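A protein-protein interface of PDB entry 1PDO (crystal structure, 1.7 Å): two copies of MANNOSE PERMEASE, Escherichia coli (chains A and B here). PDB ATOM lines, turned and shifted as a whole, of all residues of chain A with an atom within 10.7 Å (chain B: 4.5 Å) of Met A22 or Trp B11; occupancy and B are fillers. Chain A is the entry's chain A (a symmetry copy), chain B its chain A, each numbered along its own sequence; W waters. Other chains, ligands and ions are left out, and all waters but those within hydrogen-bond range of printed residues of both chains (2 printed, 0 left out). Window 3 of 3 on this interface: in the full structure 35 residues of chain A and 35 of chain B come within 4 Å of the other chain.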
ATOM      1  N   TRP A  11     -34.815  24.008  31.878  1.00  0.00           N
ATOM      2  CA  TRP A  11     -34.771  22.732  31.170  1.00  0.00           C
ATOM      3  C   TRP A  11     -33.404  22.377  30.593  1.00  0.00           C
ATOM      4  O   TRP A  11     -33.300  21.628  29.636  1.00  0.00           O
ATOM      5  CB  TRP A  11     -35.824  22.820  30.032  1.00  0.00           C
ATOM      6  CG  TRP A  11     -37.194  23.282  30.529  1.00  0.00           C
ATOM      7  CD1 TRP A  11     -38.236  22.486  30.906  1.00  0.00           C
ATOM      8  CD2 TRP A  11     -37.644  24.645  30.773  1.00  0.00           C
ATOM      9  NE1 TRP A  11     -39.286  23.246  31.365  1.00  0.00           N
ATOM     10  CE2 TRP A  11     -38.956  24.569  31.296  1.00  0.00           C
ATOM     11  CE3 TRP A  11     -37.049  25.911  30.606  1.00  0.00           C
ATOM     12  CZ2 TRP A  11     -39.704  25.700  31.649  1.00  0.00           C
ATOM     13  CZ3 TRP A  11     -37.799  27.050  30.966  1.00  0.00           C
ATOM     14  CH2 TRP A  11     -39.115  26.923  31.481  1.00  0.00           C
ATOM     15  N   ALA A  12     -32.337  22.911  31.186  1.00  0.00           N
ATOM     16  CA  ALA A  12     -31.018  22.648  30.655  1.00  0.00           C
ATOM     17  C   ALA A  12     -30.423  21.281  31.025  1.00  0.00           C
ATOM     18  O   ALA A  12     -29.548  20.808  30.307  1.00  0.00           O
ATOM     19  CB  ALA A  12     -30.044  23.774  31.059  1.00  0.00           C
ATOM     20  N   ALA A  13     -30.816  20.692  32.161  1.00  0.00           N
ATOM     21  CA  ALA A  13     -30.214  19.421  32.591  1.00  0.00           C
ATOM     22  C   ALA A  13     -30.307  18.333  31.528  1.00  0.00           C
ATOM     23  O   ALA A  13     -29.335  17.636  31.244  1.00  0.00           O
ATOM     24  CB  ALA A  13     -30.834  18.961  33.915  1.00  0.00           C
ATOM     25  N   GLU A  14     -31.481  18.176  30.933  1.00  0.00           N
ATOM     26  CA  GLU A  14     -31.664  17.150  29.905  1.00  0.00           C
ATOM     27  C   GLU A  14     -30.717  17.373  28.726  1.00  0.00           C
ATOM     28  O   GLU A  14     -30.147  16.416  28.202  1.00  0.00           O
ATOM     29  CB  GLU A  14     -33.111  17.155  29.433  1.00  0.00           C
ATOM     30  CG  GLU A  14     -33.296  16.367  28.197  1.00  0.00           C
ATOM     31  CD  GLU A  14     -34.729  16.310  27.789  1.00  0.00           C
ATOM     32  OE1 GLU A  14     -35.469  17.302  28.016  1.00  0.00           O
ATOM     33  OE2 GLU A  14     -35.108  15.246  27.261  1.00  0.00           O
ATOM     34  N   GLN A  15     -30.537  18.638  28.330  1.00  0.00           N
ATOM     35  CA  GLN A  15     -29.625  18.963  27.218  1.00  0.00           C
ATOM     36  C   GLN A  15     -28.136  18.768  27.550  1.00  0.00           C
ATOM     37  O   GLN A  15     -27.354  18.422  26.686  1.00  0.00           O
ATOM     38  CB  GLN A  15     -29.873  20.389  26.686  1.00  0.00           C
ATOM     39  CG  GLN A  15     -31.269  20.558  26.078  1.00  0.00           C
ATOM     40  CD  GLN A  15     -31.563  19.484  25.021  1.00  0.00           C
ATOM     41  OE1 GLN A  15     -30.689  19.093  24.234  1.00  0.00           O
ATOM     42  NE2 GLN A  15     -32.789  18.963  25.041  1.00  0.00           N
ATOM     43  N   LEU A  16     -27.739  19.048  28.794  1.00  0.00           N
ATOM     44  CA  LEU A  16     -26.338  18.849  29.190  1.00  0.00           C
ATOM     45  C   LEU A  16     -26.049  17.339  29.087  1.00  0.00           C
ATOM     46  O   LEU A  16     -24.970  16.926  28.695  1.00  0.00           O
ATOM     47  CB  LEU A  16     -26.118  19.352  30.622  1.00  0.00           C
ATOM     48  CG  LEU A  16     -26.197  20.857  30.909  1.00  0.00           C
ATOM     49  CD1 LEU A  16     -26.065  21.151  32.424  1.00  0.00           C
ATOM     50  CD2 LEU A  16     -25.105  21.496  30.163  1.00  0.00           C
ATOM     51  N   LEU A  17     -27.008  16.513  29.498  1.00  0.00           N
ATOM     52  CA  LEU A  17     -26.852  15.068  29.407  1.00  0.00           C
ATOM     53  C   LEU A  17     -26.773  14.659  27.922  1.00  0.00           C
ATOM     54  O   LEU A  17     -25.876  13.881  27.544  1.00  0.00           O
ATOM     55  CB  LEU A  17     -28.019  14.385  30.132  1.00  0.00           C
ATOM     56  CG  LEU A  17     -28.102  12.862  29.999  1.00  0.00           C
ATOM     57  CD1 LEU A  17     -26.737  12.237  30.334  1.00  0.00           C
ATOM     58  CD2 LEU A  17     -29.207  12.314  30.899  1.00  0.00           C
ATOM     59  N   LYS A  18     -27.644  15.242  27.083  1.00  0.00           N
ATOM     60  CA  LYS A  18     -27.675  14.911  25.652  1.00  0.00           C
ATOM     61  C   LYS A  18     -26.367  15.252  24.985  1.00  0.00           C
ATOM     62  O   LYS A  18     -25.879  14.519  24.121  1.00  0.00           O
ATOM     63  CB  LYS A  18     -28.788  15.654  24.907  1.00  0.00           C
ATOM     64  CG  LYS A  18     -30.173  15.141  25.185  1.00  0.00           C
ATOM     65  CD  LYS A  18     -31.115  15.353  24.005  1.00  0.00           C
ATOM     66  CE  LYS A  18     -32.533  15.082  24.452  1.00  0.00           C
ATOM     67  NZ  LYS A  18     -32.610  13.911  25.396  1.00  0.00           N
ATOM     68  N   THR A  19     -25.802  16.385  25.396  1.00  0.00           N
ATOM     69  CA  THR A  19     -24.536  16.842  24.871  1.00  0.00           C
ATOM     70  C   THR A  19     -23.456  15.834  25.256  1.00  0.00           C
ATOM     71  O   THR A  19     -22.627  15.424  24.415  1.00  0.00           O
ATOM     72  CB  THR A  19     -24.222  18.257  25.424  1.00  0.00           C
ATOM     73  OG1 THR A  19     -25.114  19.186  24.798  1.00  0.00           O
ATOM     74  CG2 THR A  19     -22.756  18.681  25.148  1.00  0.00           C
ATOM     75  N   ALA A  20     -23.453  15.449  26.533  1.00  0.00           N
ATOM     76  CA  ALA A  20     -22.473  14.467  26.991  1.00  0.00           C
ATOM     77  C   ALA A  20     -22.577  13.146  26.189  1.00  0.00           C
ATOM     78  O   ALA A  20     -21.569  12.548  25.804  1.00  0.00           O
ATOM     79  CB  ALA A  20     -22.647  14.204  28.508  1.00  0.00           C
ATOM     80  N   GLU A  21     -23.804  12.682  25.985  1.00  0.00           N
ATOM     81  CA  GLU A  21     -24.023  11.444  25.267  1.00  0.00           C
ATOM     82  C   GLU A  21     -23.641  11.596  23.802  1.00  0.00           C
ATOM     83  O   GLU A  21     -23.385  10.606  23.136  1.00  0.00           O
ATOM     84  CB  GLU A  21     -25.478  11.024  25.398  1.00  0.00           C
ATOM     85  CG  GLU A  21     -25.856  10.616  26.842  1.00  0.00           C
ATOM     86  CD  GLU A  21     -27.280  10.090  26.945  1.00  0.00           C
ATOM     87  OE1 GLU A  21     -28.167  10.613  26.221  1.00  0.00           O
ATOM     88  OE2 GLU A  21     -27.514   9.169  27.753  1.00  0.00           O
ATOM     89  N   MET A  22     -23.641  12.821  23.278  1.00  0.00           N
ATOM     90  CA  MET A  22     -23.247  13.012  21.890  1.00  0.00           C
ATOM     91  C   MET A  22     -21.733  12.752  21.848  1.00  0.00           C
ATOM     92  O   MET A  22     -21.196  12.200  20.882  1.00  0.00           O
ATOM     93  CB  MET A  22     -23.594  14.434  21.415  1.00  0.00           C
ATOM     94  CG  MET A  22     -22.991  14.851  20.046  1.00  0.00           C
ATOM     95  SD  MET A  22     -23.752  16.357  19.227  1.00  0.00           S
ATOM     96  CE  MET A  22     -25.474  16.182  20.163  1.00  0.00           C
ATOM     97  N   LEU A  23     -21.052  13.078  22.943  1.00  0.00           N
ATOM     98  CA  LEU A  23     -19.603  12.890  23.012  1.00  0.00           C
ATOM     99  C   LEU A  23     -19.182  11.472  23.425  1.00  0.00           C
ATOM    100  O   LEU A  23     -18.217  10.897  22.904  1.00  0.00           O
ATOM    101  CB  LEU A  23     -19.003  13.922  23.999  1.00  0.00           C
ATOM    102  CG  LEU A  23     -19.190  15.375  23.538  1.00  0.00           C
ATOM    103  CD1 LEU A  23     -18.794  16.341  24.629  1.00  0.00           C
ATOM    104  CD2 LEU A  23     -18.349  15.584  22.285  1.00  0.00           C
ATOM    105  N   LEU A  24     -19.934  10.907  24.352  1.00  0.00           N
ATOM    106  CA  LEU A  24     -19.601   9.606  24.914  1.00  0.00           C
ATOM    107  C   LEU A  24     -20.484   8.392  24.563  1.00  0.00           C
ATOM    108  O   LEU A  24     -20.111   7.263  24.889  1.00  0.00           O
ATOM    109  CB  LEU A  24     -19.598   9.760  26.457  1.00  0.00           C
ATOM    110  CG  LEU A  24     -18.660  10.748  27.158  1.00  0.00           C
ATOM    111  CD1 LEU A  24     -18.782  10.675  28.694  1.00  0.00           C
ATOM    112  CD2 LEU A  24     -17.258  10.435  26.732  1.00  0.00           C
ATOM    113  N   GLY A  25     -21.649   8.620  23.963  1.00  0.00           N
ATOM    114  CA  GLY A  25     -22.576   7.525  23.693  1.00  0.00           C
ATOM    115  C   GLY A  25     -23.594   7.564  24.834  1.00  0.00           C
ATOM    116  O   GLY A  25     -23.377   8.253  25.840  1.00  0.00           O
ATOM    117  N   GLU A  26     -24.722   6.875  24.686  1.00  0.00           N
ATOM    118  CA  GLU A  26     -25.749   6.854  25.735  1.00  0.00           C
ATOM    119  C   GLU A  26     -25.230   6.322  27.041  1.00  0.00           C
ATOM    120  O   GLU A  26     -24.507   5.325  27.109  1.00  0.00           O
ATOM    121  CB  GLU A  26     -26.966   6.043  25.330  1.00  0.00           C
ATOM    122  CG  GLU A  26     -27.857   6.772  24.356  1.00  0.00           C
ATOM    123  CD  GLU A  26     -28.932   5.874  23.800  1.00  0.00           C
ATOM    124  OE1 GLU A  26     -29.641   5.240  24.619  1.00  0.00           O
ATOM    125  OE2 GLU A  26     -29.049   5.787  22.551  1.00  0.00           O
ATOM    126  N   GLN A  27     -25.668   6.994  28.088  1.00  0.00           N
ATOM    127  CA  GLN A  27     -25.269   6.692  29.449  1.00  0.00           C
ATOM    128  C   GLN A  27     -26.355   6.006  30.245  1.00  0.00           C
ATOM    129  O   GLN A  27     -27.542   6.298  30.085  1.00  0.00           O
ATOM    130  CB  GLN A  27     -24.898   7.998  30.161  1.00  0.00           C
ATOM    131  CG  GLN A  27     -23.782   8.703  29.477  1.00  0.00           C
ATOM    132  CD  GLN A  27     -22.525   7.857  29.398  1.00  0.00           C
ATOM    133  OE1 GLN A  27     -21.987   7.447  30.420  1.00  0.00           O
ATOM    134  NE2 GLN A  27     -22.030   7.631  28.191  1.00  0.00           N
ATOM    135  N   ILE A  94     -19.775  20.912  30.853  1.00  0.00           N
ATOM    136  CA  ILE A  94     -19.477  19.736  30.049  1.00  0.00           C
ATOM    137  C   ILE A  94     -18.164  19.030  30.415  1.00  0.00           C
ATOM    138  O   ILE A  94     -18.136  17.792  30.478  1.00  0.00           O
ATOM    139  CB  ILE A  94     -19.626  19.972  28.520  1.00  0.00           C
ATOM    140  CG1 ILE A  94     -21.093  20.347  28.194  1.00  0.00           C
ATOM    141  CG2 ILE A  94     -19.307  18.689  27.776  1.00  0.00           C
ATOM    142  CD1 ILE A  94     -22.097  19.247  28.545  1.00  0.00           C
ATOM    143  N   LEU A  97     -18.914  16.916  33.383  1.00  0.00           N
ATOM    144  CA  LEU A  97     -19.779  15.787  33.062  1.00  0.00           C
ATOM    145  C   LEU A  97     -19.049  14.679  32.302  1.00  0.00           C
ATOM    146  O   LEU A  97     -19.160  13.530  32.633  1.00  0.00           O
ATOM    147  CB  LEU A  97     -21.002  16.298  32.293  1.00  0.00           C
ATOM    148  CG  LEU A  97     -22.252  15.420  32.215  1.00  0.00           C
ATOM    149  CD1 LEU A  97     -22.736  15.029  33.615  1.00  0.00           C
ATOM    150  CD2 LEU A  97     -23.328  16.183  31.478  1.00  0.00           C
ATOM    151  N   VAL A  98     -18.311  15.040  31.269  1.00  0.00           N
ATOM    152  CA  VAL A  98     -17.571  14.097  30.457  1.00  0.00           C
ATOM    153  C   VAL A  98     -16.497  13.327  31.266  1.00  0.00           C
ATOM    154  O   VAL A  98     -16.418  12.098  31.192  1.00  0.00           O
ATOM    155  CB  VAL A  98     -16.948  14.852  29.241  1.00  0.00           C
ATOM    156  CG1 VAL A  98     -15.953  13.998  28.493  1.00  0.00           C
ATOM    157  CG2 VAL A  98     -18.070  15.284  28.296  1.00  0.00           C
ATOM    158  N   LEU A 101     -18.280  11.039  33.921  1.00  0.00           N
ATOM    159  CA  LEU A 101     -18.908   9.869  33.301  1.00  0.00           C
ATOM    160  C   LEU A 101     -17.833   8.864  32.821  1.00  0.00           C
ATOM    161  O   LEU A 101     -17.996   7.663  32.945  1.00  0.00           O
ATOM    162  CB  LEU A 101     -19.832  10.283  32.135  1.00  0.00           C
ATOM    163  CG  LEU A 101     -21.059  11.097  32.544  1.00  0.00           C
ATOM    164  CD1 LEU A 101     -21.798  11.602  31.294  1.00  0.00           C
ATOM    165  CD2 LEU A 101     -21.965  10.272  33.431  1.00  0.00           C
ATOM    166  N   HIS B   9     -21.803  21.406  21.698  1.00  0.00           N
ATOM    167  CA  HIS B   9     -22.183  20.279  20.836  1.00  0.00           C
ATOM    168  C   HIS B   9     -23.680  20.091  21.133  1.00  0.00           C
ATOM    169  O   HIS B   9     -24.149  20.379  22.231  1.00  0.00           O
ATOM    170  CB  HIS B   9     -21.455  19.011  21.264  1.00  0.00           C
ATOM    171  CG  HIS B   9     -19.976  19.062  21.066  1.00  0.00           C
ATOM    172  ND1 HIS B   9     -19.133  19.755  21.911  1.00  0.00           N
ATOM    173  CD2 HIS B   9     -19.188  18.474  20.139  1.00  0.00           C
ATOM    174  CE1 HIS B   9     -17.882  19.596  21.513  1.00  0.00           C
ATOM    175  NE2 HIS B   9     -17.891  18.824  20.442  1.00  0.00           N
ATOM    176  N   GLY B  10     -24.438  19.588  20.182  1.00  0.00           N
ATOM    177  CA  GLY B  10     -25.836  19.402  20.498  1.00  0.00           C
ATOM    178  C   GLY B  10     -26.652  20.676  20.568  1.00  0.00           C
ATOM    179  O   GLY B  10     -26.369  21.631  19.845  1.00  0.00           O
ATOM    180  N   TRP B  11     -27.649  20.681  21.445  1.00  0.00           N
ATOM    181  CA  TRP B  11     -28.622  21.762  21.577  1.00  0.00           C
ATOM    182  C   TRP B  11     -28.681  22.392  22.965  1.00  0.00           C
ATOM    183  O   TRP B  11     -29.690  22.951  23.361  1.00  0.00           O
ATOM    184  CB  TRP B  11     -30.005  21.160  21.206  1.00  0.00           C
ATOM    185  CG  TRP B  11     -29.985  20.413  19.872  1.00  0.00           C
ATOM    186  CD1 TRP B  11     -30.310  20.921  18.648  1.00  0.00           C
ATOM    187  CD2 TRP B  11     -29.551  19.047  19.618  1.00  0.00           C
ATOM    188  NE1 TRP B  11     -30.107  19.982  17.663  1.00  0.00           N
ATOM    189  CE2 TRP B  11     -29.644  18.827  18.225  1.00  0.00           C
ATOM    190  CE3 TRP B  11     -29.084  18.005  20.443  1.00  0.00           C
ATOM    191  CZ2 TRP B  11     -29.303  17.609  17.619  1.00  0.00           C
ATOM    192  CZ3 TRP B  11     -28.735  16.781  19.834  1.00  0.00           C
ATOM    193  CH2 TRP B  11     -28.852  16.606  18.431  1.00  0.00           C
ATOM    194  N   ALA B  12     -27.582  22.316  23.714  1.00  0.00           N
ATOM    195  CA  ALA B  12     -27.592  22.855  25.056  1.00  0.00           C
ATOM    196  C   ALA B  12     -27.437  24.380  25.151  1.00  0.00           C
ATOM    197  O   ALA B  12     -27.849  24.950  26.156  1.00  0.00           O
ATOM    198  CB  ALA B  12     -26.519  22.161  25.921  1.00  0.00           C
ATOM    199  N   ALA B  13     -26.782  25.024  24.178  1.00  0.00           N
ATOM    200  CA  ALA B  13     -26.543  26.473  24.268  1.00  0.00           C
ATOM    201  C   ALA B  13     -27.824  27.271  24.480  1.00  0.00           C
ATOM    202  O   ALA B  13     -27.888  28.159  25.327  1.00  0.00           O
ATOM    203  CB  ALA B  13     -25.779  26.963  23.035  1.00  0.00           C
ATOM    204  N   GLU B  14     -28.857  26.962  23.708  1.00  0.00           N
ATOM    205  CA  GLU B  14     -30.125  27.682  23.837  1.00  0.00           C
ATOM    206  C   GLU B  14     -30.703  27.537  25.244  1.00  0.00           C
ATOM    207  O   GLU B  14     -31.212  28.507  25.806  1.00  0.00           O
ATOM    208  CB  GLU B  14     -31.112  27.164  22.800  1.00  0.00           C
ATOM    209  CG  GLU B  14     -32.491  27.622  23.068  1.00  0.00           C
ATOM    210  CD  GLU B  14     -33.435  27.178  22.002  1.00  0.00           C
ATOM    211  OE1 GLU B  14     -33.241  26.070  21.437  1.00  0.00           O
ATOM    212  OE2 GLU B  14     -34.359  27.966  21.723  1.00  0.00           O
ATOM    213  N   GLN B  15     -30.601  26.331  25.815  1.00  0.00           N
ATOM    214  CA  GLN B  15     -31.105  26.092  27.180  1.00  0.00           C
ATOM    215  C   GLN B  15     -30.279  26.775  28.283  1.00  0.00           C
ATOM    216  O   GLN B  15     -30.818  27.173  29.297  1.00  0.00           O
ATOM    217  CB  GLN B  15     -31.245  24.585  27.471  1.00  0.00           C
ATOM    218  CG  GLN B  15     -32.281  23.902  26.572  1.00  0.00           C
ATOM    219  CD  GLN B  15     -33.633  24.630  26.609  1.00  0.00           C
ATOM    220  OE1 GLN B  15     -34.081  25.110  27.660  1.00  0.00           O
ATOM    221  NE2 GLN B  15     -34.259  24.759  25.442  1.00  0.00           N
ATOM    222  N   ASP B  34     -26.110  25.732  17.481  1.00  0.00           N
ATOM    223  CA  ASP B  34     -26.095  24.317  17.807  1.00  0.00           C
ATOM    224  C   ASP B  34     -25.122  23.592  16.892  1.00  0.00           C
ATOM    225  O   ASP B  34     -24.644  24.145  15.912  1.00  0.00           O
ATOM    226  CB  ASP B  34     -27.499  23.664  17.864  1.00  0.00           C
ATOM    227  CG  ASP B  34     -28.406  24.067  16.747  1.00  0.00           C
ATOM    228  OD1 ASP B  34     -27.939  24.068  15.597  1.00  0.00           O
ATOM    229  OD2 ASP B  34     -29.595  24.357  17.034  1.00  0.00           O
ATOM    230  N   PHE B  35     -24.727  22.389  17.273  1.00  0.00           N
ATOM    231  CA  PHE B  35     -23.819  21.618  16.472  1.00  0.00           C
ATOM    232  C   PHE B  35     -24.381  20.207  16.402  1.00  0.00           C
ATOM    233  O   PHE B  35     -24.557  19.525  17.411  1.00  0.00           O
ATOM    234  CB  PHE B  35     -22.410  21.688  17.057  1.00  0.00           C
ATOM    235  CG  PHE B  35     -21.407  20.786  16.381  1.00  0.00           C
ATOM    236  CD1 PHE B  35     -21.275  20.741  14.993  1.00  0.00           C
ATOM    237  CD2 PHE B  35     -20.589  19.964  17.141  1.00  0.00           C
ATOM    238  CE1 PHE B  35     -20.349  19.881  14.390  1.00  0.00           C
ATOM    239  CE2 PHE B  35     -19.664  19.104  16.537  1.00  0.00           C
ATOM    240  CZ  PHE B  35     -19.549  19.064  15.158  1.00  0.00           C
ATOM    241  N   VAL B  36     -24.701  19.815  15.178  1.00  0.00           N
ATOM    242  CA  VAL B  36     -25.326  18.533  14.884  1.00  0.00           C
ATOM    243  C   VAL B  36     -24.334  17.586  14.202  1.00  0.00           C
ATOM    244  O   VAL B  36     -23.483  18.037  13.426  1.00  0.00           O
ATOM    245  CB  VAL B  36     -26.593  18.786  13.958  1.00  0.00           C
ATOM    246  CG1 VAL B  36     -27.269  17.491  13.575  1.00  0.00           C
ATOM    247  CG2 VAL B  36     -27.586  19.683  14.675  1.00  0.00           C
ATOM    248  N   PRO B  37     -24.422  16.266  14.478  1.00  0.00           N
ATOM    249  CA  PRO B  37     -23.502  15.310  13.843  1.00  0.00           C
ATOM    250  C   PRO B  37     -23.644  15.457  12.326  1.00  0.00           C
ATOM    251  O   PRO B  37     -24.768  15.527  11.821  1.00  0.00           O
ATOM    252  CB  PRO B  37     -24.061  13.970  14.304  1.00  0.00           C
ATOM    253  CG  PRO B  37     -24.585  14.292  15.644  1.00  0.00           C
ATOM    254  CD  PRO B  37     -25.340  15.561  15.386  1.00  0.00           C
HETATM  255  O   HOH W   1     -33.620  25.991  30.082  1.00  0.00           O
HETATM  256  O   HOH W   2     -28.143  18.847  23.676  1.00  0.00           O
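O of His B9 is in hydrogen-bond range of OG1 of Thr A19, at 3.0 Å.
SD of Met A22 lies close to O of Phe B35 (3.7 Å).
N of Gly B10 lies within hydrogen-bond range of SD of Met A22, at 3.4 Å.
The backbone NH of Gly B10 is in hydrogen-bond range of the backbone carbonyl oxygen of Phe B35 (2.8 Å).
The side-chain hydroxyl (OG1) of Thr A19 lies within hydrogen-bond range of the backbone carbonyl oxygen (O) of Gln A15, at 3.0 Å.
OE1 of Gln B15 touches CB of Trp A11, 3.7 Å away.
Ala A12 touches Gln B15 (CA to CB, 3.7 Å).
Gln A15 touches Trp B11 (OE1 to CB, 3.7 Å).
Gln A15 touches Ala B12.
Gln A15 touches Gln B15 (CG to CG, 3.5 Å).
CB of Ala B12 touches OG1 of Thr A19 (3.5 Å).
Trp B11 touches Met A22 (CZ3 to CE, 3.3 Å).
His B9 touches Leu A23 (CD2 to CD2, 3.7 Å).
Printed residues of chain B within 4 Å of Met A22: Gly B10 (3.3 Å), Trp B11 (3.3 Å) and Phe B35 (3.7 Å).
Of chain A, only Gln A15 (3.7 Å) and Met A22 (3.3 Å) come within 4 Å of Trp B11.
Of chain A, only Met A22 (3.3 Å) comes within 4 Å of Gly B10.
No residue of chain A comes within 4 Å of Val B36.
Of the printed residues of chain B, Trp A11 touches Gln B15 (3.7 Å).
Printed residues of chain A within 4 Å of Phe B35: Met A22 (3.7 Å).
Lys A18 touches none of the printed residues of chain B.
The nearest residue of chain B that does not touch Met A22 is His B9 (4.1 Å).
The nearest printed residue of chain B that does not touch Leu A23 is Phe B35 (6.9 Å).
Hydrophobic or aromatic side chains of chain A within 4 Å of the printed part of chain B: Trp A11, Ala A12, Met A22 and Leu A23.
Printed residues of chain B that touch a printed residue of chain A: His B9, Gly B10, Trp B11, Ala B12, Gln B15 and Phe B35.
Hydrophobic or aromatic side chains of chain B within 4 Å of the printed part of chain A: His B9, Trp B11 and Ala B12.
Among the printed residues, no Asp or Glu carboxylate lies within 4 Å of a Lys or Arg side-chain nitrogen of the other chain.
Trp A11 touches Gln B15, and with the chains exchanged Gln A15 touches Trp B11.
Ala A12 touches Gln B15, and with the chains exchanged Gln A15 touches Ala B12.
Gln B15 touches its own counterpart, Gln A15.
Positions printed for both chains: 11, 12, 13, 14 and 15.
Of the 11 pairs that touch across the chains among the printed residues, 5 have their exchanged pair printed and touching as well.
Water W2 lies within hydrogen-bond range of OE1 of Gln A15, N of Trp B11 and OG1 of Thr A19.
Water W1 lies within hydrogen-bond range of the side-chain amide oxygen (OE1) of Gln B15 (2.6 Å) and the backbone NH (N) of Trp A11 (2.9 Å).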
